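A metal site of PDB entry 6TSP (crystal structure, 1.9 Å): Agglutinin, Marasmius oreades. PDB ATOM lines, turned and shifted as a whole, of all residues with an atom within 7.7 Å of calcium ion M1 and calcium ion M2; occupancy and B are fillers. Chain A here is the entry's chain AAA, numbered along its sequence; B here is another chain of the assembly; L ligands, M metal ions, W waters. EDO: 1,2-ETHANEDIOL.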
ATOM      1  N   TRP A 208      -1.073  -0.860  13.638  1.00  0.00           N
ATOM      2  CA  TRP A 208      -0.756  -2.299  13.513  1.00  0.00           C
ATOM      3  C   TRP A 208       0.754  -2.471  13.364  1.00  0.00           C
ATOM      4  O   TRP A 208       1.322  -1.843  12.492  1.00  0.00           O
ATOM      5  CB  TRP A 208      -1.512  -2.910  12.325  1.00  0.00           C
ATOM      6  CG  TRP A 208      -1.327  -4.391  12.184  1.00  0.00           C
ATOM      7  CD1 TRP A 208      -2.160  -5.377  12.643  1.00  0.00           C
ATOM      8  CD2 TRP A 208      -0.215  -5.071  11.573  1.00  0.00           C
ATOM      9  NE1 TRP A 208      -1.653  -6.611  12.345  1.00  0.00           N
ATOM     10  CE2 TRP A 208      -0.463  -6.458  11.670  1.00  0.00           C
ATOM     11  CE3 TRP A 208       0.952  -4.644  10.910  1.00  0.00           C
ATOM     12  CZ2 TRP A 208       0.405  -7.409  11.154  1.00  0.00           C
ATOM     13  CZ3 TRP A 208       1.819  -5.599  10.414  1.00  0.00           C
ATOM     14  CH2 TRP A 208       1.546  -6.956  10.536  1.00  0.00           C
ATOM     15  N   ARG A 209       1.353  -3.282  14.229  1.00  0.00           N
ATOM     16  CA  ARG A 209       2.787  -3.659  14.137  1.00  0.00           C
ATOM     17  C   ARG A 209       2.929  -5.176  14.353  1.00  0.00           C
ATOM     18  O   ARG A 209       2.232  -5.733  15.263  1.00  0.00           O
ATOM     19  CB  ARG A 209       3.608  -2.858  15.152  1.00  0.00           C
ATOM     20  CG  ARG A 209       3.464  -1.346  15.006  1.00  0.00           C
ATOM     21  CD  ARG A 209       4.094  -0.563  16.200  1.00  0.00           C
ATOM     22  NE  ARG A 209       5.467  -0.963  16.426  1.00  0.00           N
ATOM     23  CZ  ARG A 209       6.149  -0.745  17.573  1.00  0.00           C
ATOM     24  NH1 ARG A 209       5.623  -0.023  18.533  1.00  0.00           N
ATOM     25  NH2 ARG A 209       7.380  -1.198  17.698  1.00  0.00           N
ATOM     26  N   GLU A 210       3.673  -5.827  13.481  1.00  0.00           N
ATOM     27  CA  GLU A 210       3.797  -7.299  13.461  1.00  0.00           C
ATOM     28  C   GLU A 210       4.153  -7.819  14.869  1.00  0.00           C
ATOM     29  O   GLU A 210       5.232  -7.421  15.411  1.00  0.00           O
ATOM     30  CB  GLU A 210       4.862  -7.705  12.442  1.00  0.00           C
ATOM     31  CG  GLU A 210       4.804  -9.148  12.069  1.00  0.00           C
ATOM     32  CD  GLU A 210       5.940  -9.594  11.169  1.00  0.00           C
ATOM     33  OE1 GLU A 210       6.341 -10.766  11.276  1.00  0.00           O
ATOM     34  OE2 GLU A 210       6.463  -8.742  10.420  1.00  0.00           O
ATOM     35  N   GLN A 211       3.239  -8.598  15.467  1.00  0.00           N
ATOM     36  CA  GLN A 211       3.376  -9.291  16.777  1.00  0.00           C
ATOM     37  C   GLN A 211       3.326  -8.241  17.933  1.00  0.00           C
ATOM     38  O   GLN A 211       2.696  -8.529  18.931  1.00  0.00           O
ATOM     39  CB  GLN A 211       4.669 -10.126  16.820  1.00  0.00           C
ATOM     40  CG  GLN A 211       4.627 -11.348  15.879  1.00  0.00           C
ATOM     41  CD  GLN A 211       5.650 -12.415  16.248  1.00  0.00           C
ATOM     42  OE1 GLN A 211       5.749 -12.815  17.400  1.00  0.00           O
ATOM     43  NE2 GLN A 211       6.417 -12.869  15.263  1.00  0.00           N
ATOM     44  N   ILE A 212       4.066  -7.140  17.808  1.00  0.00           N
ATOM     45  CA  ILE A 212       4.294  -6.226  18.985  1.00  0.00           C
ATOM     46  C   ILE A 212       2.986  -5.438  19.279  1.00  0.00           C
ATOM     47  O   ILE A 212       2.755  -5.088  20.468  1.00  0.00           O
ATOM     48  CB  ILE A 212       5.492  -5.290  18.742  1.00  0.00           C
ATOM     49  CG1 ILE A 212       5.889  -4.530  20.030  1.00  0.00           C
ATOM     50  CG2 ILE A 212       5.220  -4.355  17.605  1.00  0.00           C
ATOM     51  CD1 ILE A 212       6.278  -5.440  21.179  1.00  0.00           C
ATOM     52  N   TYR A 213       2.220  -5.130  18.243  1.00  0.00           N
ATOM     53  CA  TYR A 213       0.830  -4.584  18.432  1.00  0.00           C
ATOM     54  C   TYR A 213      -0.014  -4.940  17.208  1.00  0.00           C
ATOM     55  O   TYR A 213      -0.272  -4.066  16.346  1.00  0.00           O
ATOM     56  CB  TYR A 213       0.871  -3.088  18.672  1.00  0.00           C
ATOM     57  CG  TYR A 213      -0.111  -2.628  19.696  1.00  0.00           C
ATOM     58  CD1 TYR A 213       0.057  -2.937  21.034  1.00  0.00           C
ATOM     59  CD2 TYR A 213      -1.287  -1.988  19.325  1.00  0.00           C
ATOM     60  CE1 TYR A 213      -0.872  -2.568  21.992  1.00  0.00           C
ATOM     61  CE2 TYR A 213      -2.232  -1.601  20.265  1.00  0.00           C
ATOM     62  CZ  TYR A 213      -2.033  -1.906  21.605  1.00  0.00           C
ATOM     63  OH  TYR A 213      -2.959  -1.526  22.556  1.00  0.00           O
ATOM     64  N   ASP A 214      -0.439  -6.164  17.154  1.00  0.00           N
ATOM     65  CA  ASP A 214      -1.231  -6.698  16.030  1.00  0.00           C
ATOM     66  C   ASP A 214      -2.594  -7.094  16.595  1.00  0.00           C
ATOM     67  O   ASP A 214      -3.010  -6.478  17.602  1.00  0.00           O
ATOM     68  CB  ASP A 214      -0.496  -7.856  15.342  1.00  0.00           C
ATOM     69  CG  ASP A 214      -0.273  -9.081  16.224  1.00  0.00           C
ATOM     70  OD1 ASP A 214      -0.130  -8.892  17.455  1.00  0.00           O
ATOM     71  OD2 ASP A 214      -0.215 -10.189  15.680  1.00  0.00           O
ATOM     72  N   CYS A 215      -3.355  -7.884  15.862  1.00  0.00           N
ATOM     73  CA  CYS A 215      -4.826  -7.953  16.077  1.00  0.00           C
ATOM     74  C   CYS A 215      -5.137  -8.434  17.526  1.00  0.00           C
ATOM     75  O   CYS A 215      -6.000  -7.830  18.146  1.00  0.00           O
ATOM     76  CB  CYS A 215      -5.527  -8.868  15.036  1.00  0.00           C
ATOM     77  SG  CYS A 215      -4.684 -10.443  14.731  1.00  0.00           S
ATOM     78  N   ASP A 216      -4.357  -9.382  18.067  1.00  0.00           N
ATOM     79  CA  ASP A 216      -4.602  -9.889  19.474  1.00  0.00           C
ATOM     80  C   ASP A 216      -4.476  -8.700  20.484  1.00  0.00           C
ATOM     81  O   ASP A 216      -5.314  -8.627  21.419  1.00  0.00           O
ATOM     82  CB  ASP A 216      -3.694 -11.065  19.834  1.00  0.00           C
ATOM     83  CG  ASP A 216      -2.225 -10.817  19.562  1.00  0.00           C
ATOM     84  OD1 ASP A 216      -1.792 -11.078  18.443  1.00  0.00           O
ATOM     85  OD2 ASP A 216      -1.527 -10.355  20.482  1.00  0.00           O
ATOM     86  N   ASP A 217      -3.579  -7.735  20.209  1.00  0.00           N
ATOM     87  CA  ASP A 217      -3.290  -6.604  21.136  1.00  0.00           C
ATOM     88  C   ASP A 217      -4.432  -5.590  21.086  1.00  0.00           C
ATOM     89  O   ASP A 217      -4.875  -5.142  22.171  1.00  0.00           O
ATOM     90  CB  ASP A 217      -1.949  -5.959  20.792  1.00  0.00           C
ATOM     91  CG  ASP A 217      -0.779  -6.877  21.005  1.00  0.00           C
ATOM     92  OD1 ASP A 217      -0.405  -7.092  22.190  1.00  0.00           O
ATOM     93  OD2 ASP A 217      -0.385  -7.546  20.027  1.00  0.00           O
ATOM     94  N   PHE A 218      -4.998  -5.364  19.893  1.00  0.00           N
ATOM     95  CA  PHE A 218      -6.172  -4.463  19.717  1.00  0.00           C
ATOM     96  C   PHE A 218      -7.387  -5.062  20.455  1.00  0.00           C
ATOM     97  O   PHE A 218      -8.041  -4.337  21.183  1.00  0.00           O
ATOM     98  CB  PHE A 218      -6.470  -4.252  18.229  1.00  0.00           C
ATOM     99  CG  PHE A 218      -5.620  -3.204  17.559  1.00  0.00           C
ATOM    100  CD1 PHE A 218      -4.350  -3.515  17.072  1.00  0.00           C
ATOM    101  CD2 PHE A 218      -6.109  -1.924  17.326  1.00  0.00           C
ATOM    102  CE1 PHE A 218      -3.579  -2.550  16.431  1.00  0.00           C
ATOM    103  CE2 PHE A 218      -5.330  -0.965  16.705  1.00  0.00           C
ATOM    104  CZ  PHE A 218      -4.083  -1.291  16.213  1.00  0.00           C
ATOM    105  N   ILE A 220      -7.668  -7.378  22.846  1.00  0.00           N
ATOM    106  CA  ILE A 220      -7.506  -7.513  24.310  1.00  0.00           C
ATOM    107  C   ILE A 220      -7.511  -6.105  24.958  1.00  0.00           C
ATOM    108  O   ILE A 220      -8.171  -5.954  25.991  1.00  0.00           O
ATOM    109  CB  ILE A 220      -6.227  -8.294  24.649  1.00  0.00           C
ATOM    110  CG1 ILE A 220      -6.425  -9.800  24.470  1.00  0.00           C
ATOM    111  CG2 ILE A 220      -5.743  -7.932  26.057  1.00  0.00           C
ATOM    112  CD1 ILE A 220      -5.163 -10.563  24.249  1.00  0.00           C
ATOM    113  N   ALA A 256      -5.249 -16.562  10.873  1.00  0.00           N
ATOM    114  CA  ALA A 256      -6.050 -16.297  12.094  1.00  0.00           C
ATOM    115  C   ALA A 256      -6.099 -14.788  12.362  1.00  0.00           C
ATOM    116  O   ALA A 256      -5.182 -14.075  11.925  1.00  0.00           O
ATOM    117  CB  ALA A 256      -5.475 -17.052  13.265  1.00  0.00           C
ATOM    118  N   ALA A 258      -7.719 -11.849  15.476  1.00  0.00           N
ATOM    119  CA  ALA A 258      -8.400 -11.539  16.764  1.00  0.00           C
ATOM    120  C   ALA A 258      -9.313 -10.327  16.584  1.00  0.00           C
ATOM    121  O   ALA A 258      -8.954  -9.428  15.824  1.00  0.00           O
ATOM    122  CB  ALA A 258      -7.384 -11.302  17.832  1.00  0.00           C
ATOM    123  N   ILE B 181      -2.469 -19.574  21.428  1.00  0.00           N
ATOM    124  CA  ILE B 181      -1.198 -18.873  21.092  1.00  0.00           C
ATOM    125  C   ILE B 181      -1.520 -17.678  20.208  1.00  0.00           C
ATOM    126  O   ILE B 181      -2.287 -17.846  19.250  1.00  0.00           O
ATOM    127  CB  ILE B 181      -0.228 -19.841  20.405  1.00  0.00           C
ATOM    128  CG1 ILE B 181       0.308 -20.891  21.381  1.00  0.00           C
ATOM    129  CG2 ILE B 181       0.897 -19.084  19.703  1.00  0.00           C
ATOM    130  CD1 ILE B 181       0.286 -22.319  20.850  1.00  0.00           C
ATOM    131  N   LEU B 182      -0.999 -16.513  20.542  1.00  0.00           N
ATOM    132  CA  LEU B 182      -1.368 -15.233  19.897  1.00  0.00           C
ATOM    133  C   LEU B 182      -0.219 -14.761  18.987  1.00  0.00           C
ATOM    134  O   LEU B 182      -0.496 -14.031  18.033  1.00  0.00           O
ATOM    135  CB  LEU B 182      -1.678 -14.210  20.992  1.00  0.00           C
ATOM    136  CG  LEU B 182      -2.834 -14.570  21.924  1.00  0.00           C
ATOM    137  CD1 LEU B 182      -2.999 -13.536  23.019  1.00  0.00           C
ATOM    138  CD2 LEU B 182      -4.128 -14.748  21.148  1.00  0.00           C
ATOM    139  N   ASP B 183       1.018 -15.070  19.356  1.00  0.00           N
ATOM    140  CA  ASP B 183       2.231 -14.523  18.669  1.00  0.00           C
ATOM    141  C   ASP B 183       3.260 -15.653  18.494  1.00  0.00           C
ATOM    142  O   ASP B 183       2.933 -16.815  18.836  1.00  0.00           O
ATOM    143  CB  ASP B 183       2.794 -13.321  19.432  1.00  0.00           C
ATOM    144  CG  ASP B 183       1.827 -12.105  19.484  1.00  0.00           C
ATOM    145  OD1 ASP B 183       1.479 -11.571  18.396  1.00  0.00           O
ATOM    146  OD2 ASP B 183       1.516 -11.653  20.618  1.00  0.00           O
ATOM    147  N   GLY B 184       4.444 -15.327  17.945  1.00  0.00           N
ATOM    148  CA  GLY B 184       5.452 -16.331  17.539  1.00  0.00           C
ATOM    149  C   GLY B 184       6.691 -16.305  18.445  1.00  0.00           C
ATOM    150  O   GLY B 184       7.317 -17.333  18.584  1.00  0.00           O
ATOM    151  N   TYR B 186       8.543 -14.183  21.859  1.00  0.00           N
ATOM    152  CA  TYR B 186       8.256 -13.330  23.043  1.00  0.00           C
ATOM    153  C   TYR B 186       9.563 -13.002  23.789  1.00  0.00           C
ATOM    154  O   TYR B 186      10.208 -13.958  24.310  1.00  0.00           O
ATOM    155  CB  TYR B 186       7.284 -14.023  23.981  1.00  0.00           C
ATOM    156  CG  TYR B 186       6.015 -14.506  23.340  1.00  0.00           C
ATOM    157  CD1 TYR B 186       5.926 -15.774  22.765  1.00  0.00           C
ATOM    158  CD2 TYR B 186       4.847 -13.742  23.413  1.00  0.00           C
ATOM    159  CE1 TYR B 186       4.724 -16.261  22.270  1.00  0.00           C
ATOM    160  CE2 TYR B 186       3.648 -14.222  22.929  1.00  0.00           C
ATOM    161  CZ  TYR B 186       3.580 -15.485  22.357  1.00  0.00           C
ATOM    162  OH  TYR B 186       2.391 -15.960  21.895  1.00  0.00           O
ATOM    163  N   LYS B 223      -2.429  -8.109  31.223  1.00  0.00           N
ATOM    164  CA  LYS B 223      -1.969  -8.503  29.865  1.00  0.00           C
ATOM    165  C   LYS B 223      -1.987  -7.276  28.923  1.00  0.00           C
ATOM    166  O   LYS B 223      -1.063  -7.128  28.139  1.00  0.00           O
ATOM    167  CB  LYS B 223      -2.826  -9.628  29.283  1.00  0.00           C
ATOM    168  CG  LYS B 223      -2.415 -10.064  27.872  1.00  0.00           C
ATOM    169  CD  LYS B 223      -2.522 -11.533  27.624  1.00  0.00           C
ATOM    170  CE  LYS B 223      -2.005 -11.947  26.255  1.00  0.00           C
ATOM    171  NZ  LYS B 223      -0.555 -11.635  26.096  1.00  0.00           N
ATOM    172  N   GLY B 227       1.132  -5.573  26.935  1.00  0.00           N
ATOM    173  CA  GLY B 227       0.967  -5.264  25.496  1.00  0.00           C
ATOM    174  C   GLY B 227       1.297  -3.798  25.195  1.00  0.00           C
ATOM    175  O   GLY B 227       2.096  -3.533  24.232  1.00  0.00           O
ATOM    176  N   PHE B 239       8.128  -9.286  17.141  1.00  0.00           N
ATOM    177  CA  PHE B 239       8.097 -10.047  18.397  1.00  0.00           C
ATOM    178  C   PHE B 239       6.983  -9.499  19.288  1.00  0.00           C
ATOM    179  O   PHE B 239       6.561  -8.336  19.046  1.00  0.00           O
ATOM    180  CB  PHE B 239       9.446  -9.950  19.109  1.00  0.00           C
ATOM    181  CG  PHE B 239       9.775  -8.574  19.577  1.00  0.00           C
ATOM    182  CD1 PHE B 239      10.056  -7.573  18.660  1.00  0.00           C
ATOM    183  CD2 PHE B 239       9.634  -8.222  20.915  1.00  0.00           C
ATOM    184  CE1 PHE B 239      10.197  -6.262  19.082  1.00  0.00           C
ATOM    185  CE2 PHE B 239       9.815  -6.918  21.329  1.00  0.00           C
ATOM    186  CZ  PHE B 239      10.101  -5.940  20.418  1.00  0.00           C
ATOM    187  N   ALA B 240       6.738 -10.173  20.396  1.00  0.00           N
ATOM    188  CA  ALA B 240       5.793  -9.727  21.450  1.00  0.00           C
ATOM    189  C   ALA B 240       6.489  -9.766  22.811  1.00  0.00           C
ATOM    190  O   ALA B 240       7.637 -10.273  22.880  1.00  0.00           O
ATOM    191  CB  ALA B 240       4.582 -10.606  21.438  1.00  0.00           C
ATOM    192  N   ILE B 241       5.796  -9.340  23.856  1.00  0.00           N
ATOM    193  CA  ILE B 241       6.242  -9.486  25.284  1.00  0.00           C
ATOM    194  C   ILE B 241       5.484 -10.635  25.898  1.00  0.00           C
ATOM    195  O   ILE B 241       4.258 -10.686  25.734  1.00  0.00           O
ATOM    196  CB  ILE B 241       6.015  -8.195  26.069  1.00  0.00           C
ATOM    197  CG1 ILE B 241       6.428  -6.954  25.268  1.00  0.00           C
ATOM    198  CG2 ILE B 241       6.725  -8.265  27.414  1.00  0.00           C
ATOM    199  CD1 ILE B 241       7.889  -6.947  24.815  1.00  0.00           C
ATOM    200  N   TYR B 293      -1.727 -16.423  25.522  1.00  0.00           N
ATOM    201  CA  TYR B 293      -0.420 -15.757  25.661  1.00  0.00           C
ATOM    202  C   TYR B 293       0.127 -15.463  24.271  1.00  0.00           C
ATOM    203  O   TYR B 293       0.851 -14.488  24.069  1.00  0.00           O
ATOM    204  CB  TYR B 293       0.552 -16.649  26.439  1.00  0.00           C
ATOM    205  CG  TYR B 293       0.663 -18.078  25.926  1.00  0.00           C
ATOM    206  CD1 TYR B 293      -0.212 -19.070  26.361  1.00  0.00           C
ATOM    207  CD2 TYR B 293       1.683 -18.445  25.066  1.00  0.00           C
ATOM    208  CE1 TYR B 293      -0.060 -20.396  25.963  1.00  0.00           C
ATOM    209  CE2 TYR B 293       1.818 -19.756  24.618  1.00  0.00           C
ATOM    210  CZ  TYR B 293       0.955 -20.738  25.086  1.00  0.00           C
ATOM    211  OH  TYR B 293       1.111 -22.042  24.682  1.00  0.00           O
ATOM    212  OXT TYR B 293      -0.166 -16.184  23.333  1.00  0.00           O
HETATM  213  C1  EDO L   1      -4.116 -13.680  16.929  1.00  0.00           C
HETATM  214  O1  EDO L   1      -4.703 -14.907  17.344  1.00  0.00           O
HETATM  215  C2  EDO L   1      -3.287 -13.822  15.693  1.00  0.00           C
HETATM  216  O2  EDO L   1      -2.321 -12.809  15.564  1.00  0.00           O
HETATM  217 CA    CA M   1       0.612  -9.509  19.624  1.00  0.00          CA
HETATM  218 CA    CA M   2      -0.407 -12.131  16.906  1.00  0.00          CA
HETATM  219 ZN    ZN M   3      -5.257  -9.999  12.467  1.00  0.00          ZN
HETATM  220  O   HOH W   1       1.156  -9.140  21.874  1.00  0.00           O
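N of Asp 183 of chain B sits at hydrogen-bond distance from OH of Tyr 186 of chain B. The side-chain amide oxygen (OE1) of Gln 211 lies within hydrogen-bond range of the backbone NH (N) of Gly 184 of chain B (2.9 Å). N of Leu 182 of chain B sits at hydrogen-bond distance from OXT of Tyr 293 of chain B (2.9 Å). O of Arg 209 lies within hydrogen-bond range of N of Asp 214.
Of the 25 residues printed, 5 come within 4 Å of calcium ion M1.
The nearest printed residue that does not touch calcium ion M2 is Gln 211 (4.7 Å).
Calcium ion M1 is bound by the side-chain carboxylate (OD2) of Asp 217 (2.2 Å), water W1 (2.3 Å), the side-chain carboxylate (OD1) of Asp 214 (2.4 Å), the backbone carbonyl oxygen (O) of Gln 211 (2.4 Å), the side-chain carboxylate (OD2) of Asp 216 (2.5 Å), the side-chain carboxylate (OD2) of Asp 183 of chain B (2.5 Å) and the side-chain carboxylate (OD1) of Asp 183 of chain B (2.6 Å). Slightly farther from calcium ion M1 lies OD1 of Asp 216 (3.1 Å).
O of Leu 182 of chain B is bound to calcium ion M2. OD2 of Asp 214 is bound to calcium ion M2, 2.3 Å away. The side-chain carboxylate (OD1) of Asp 216 is bound to calcium ion M2 (2.3 Å). O2 of the ligand binds calcium ion M2. OD1 of Asp 183 of chain B binds calcium ion M2.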
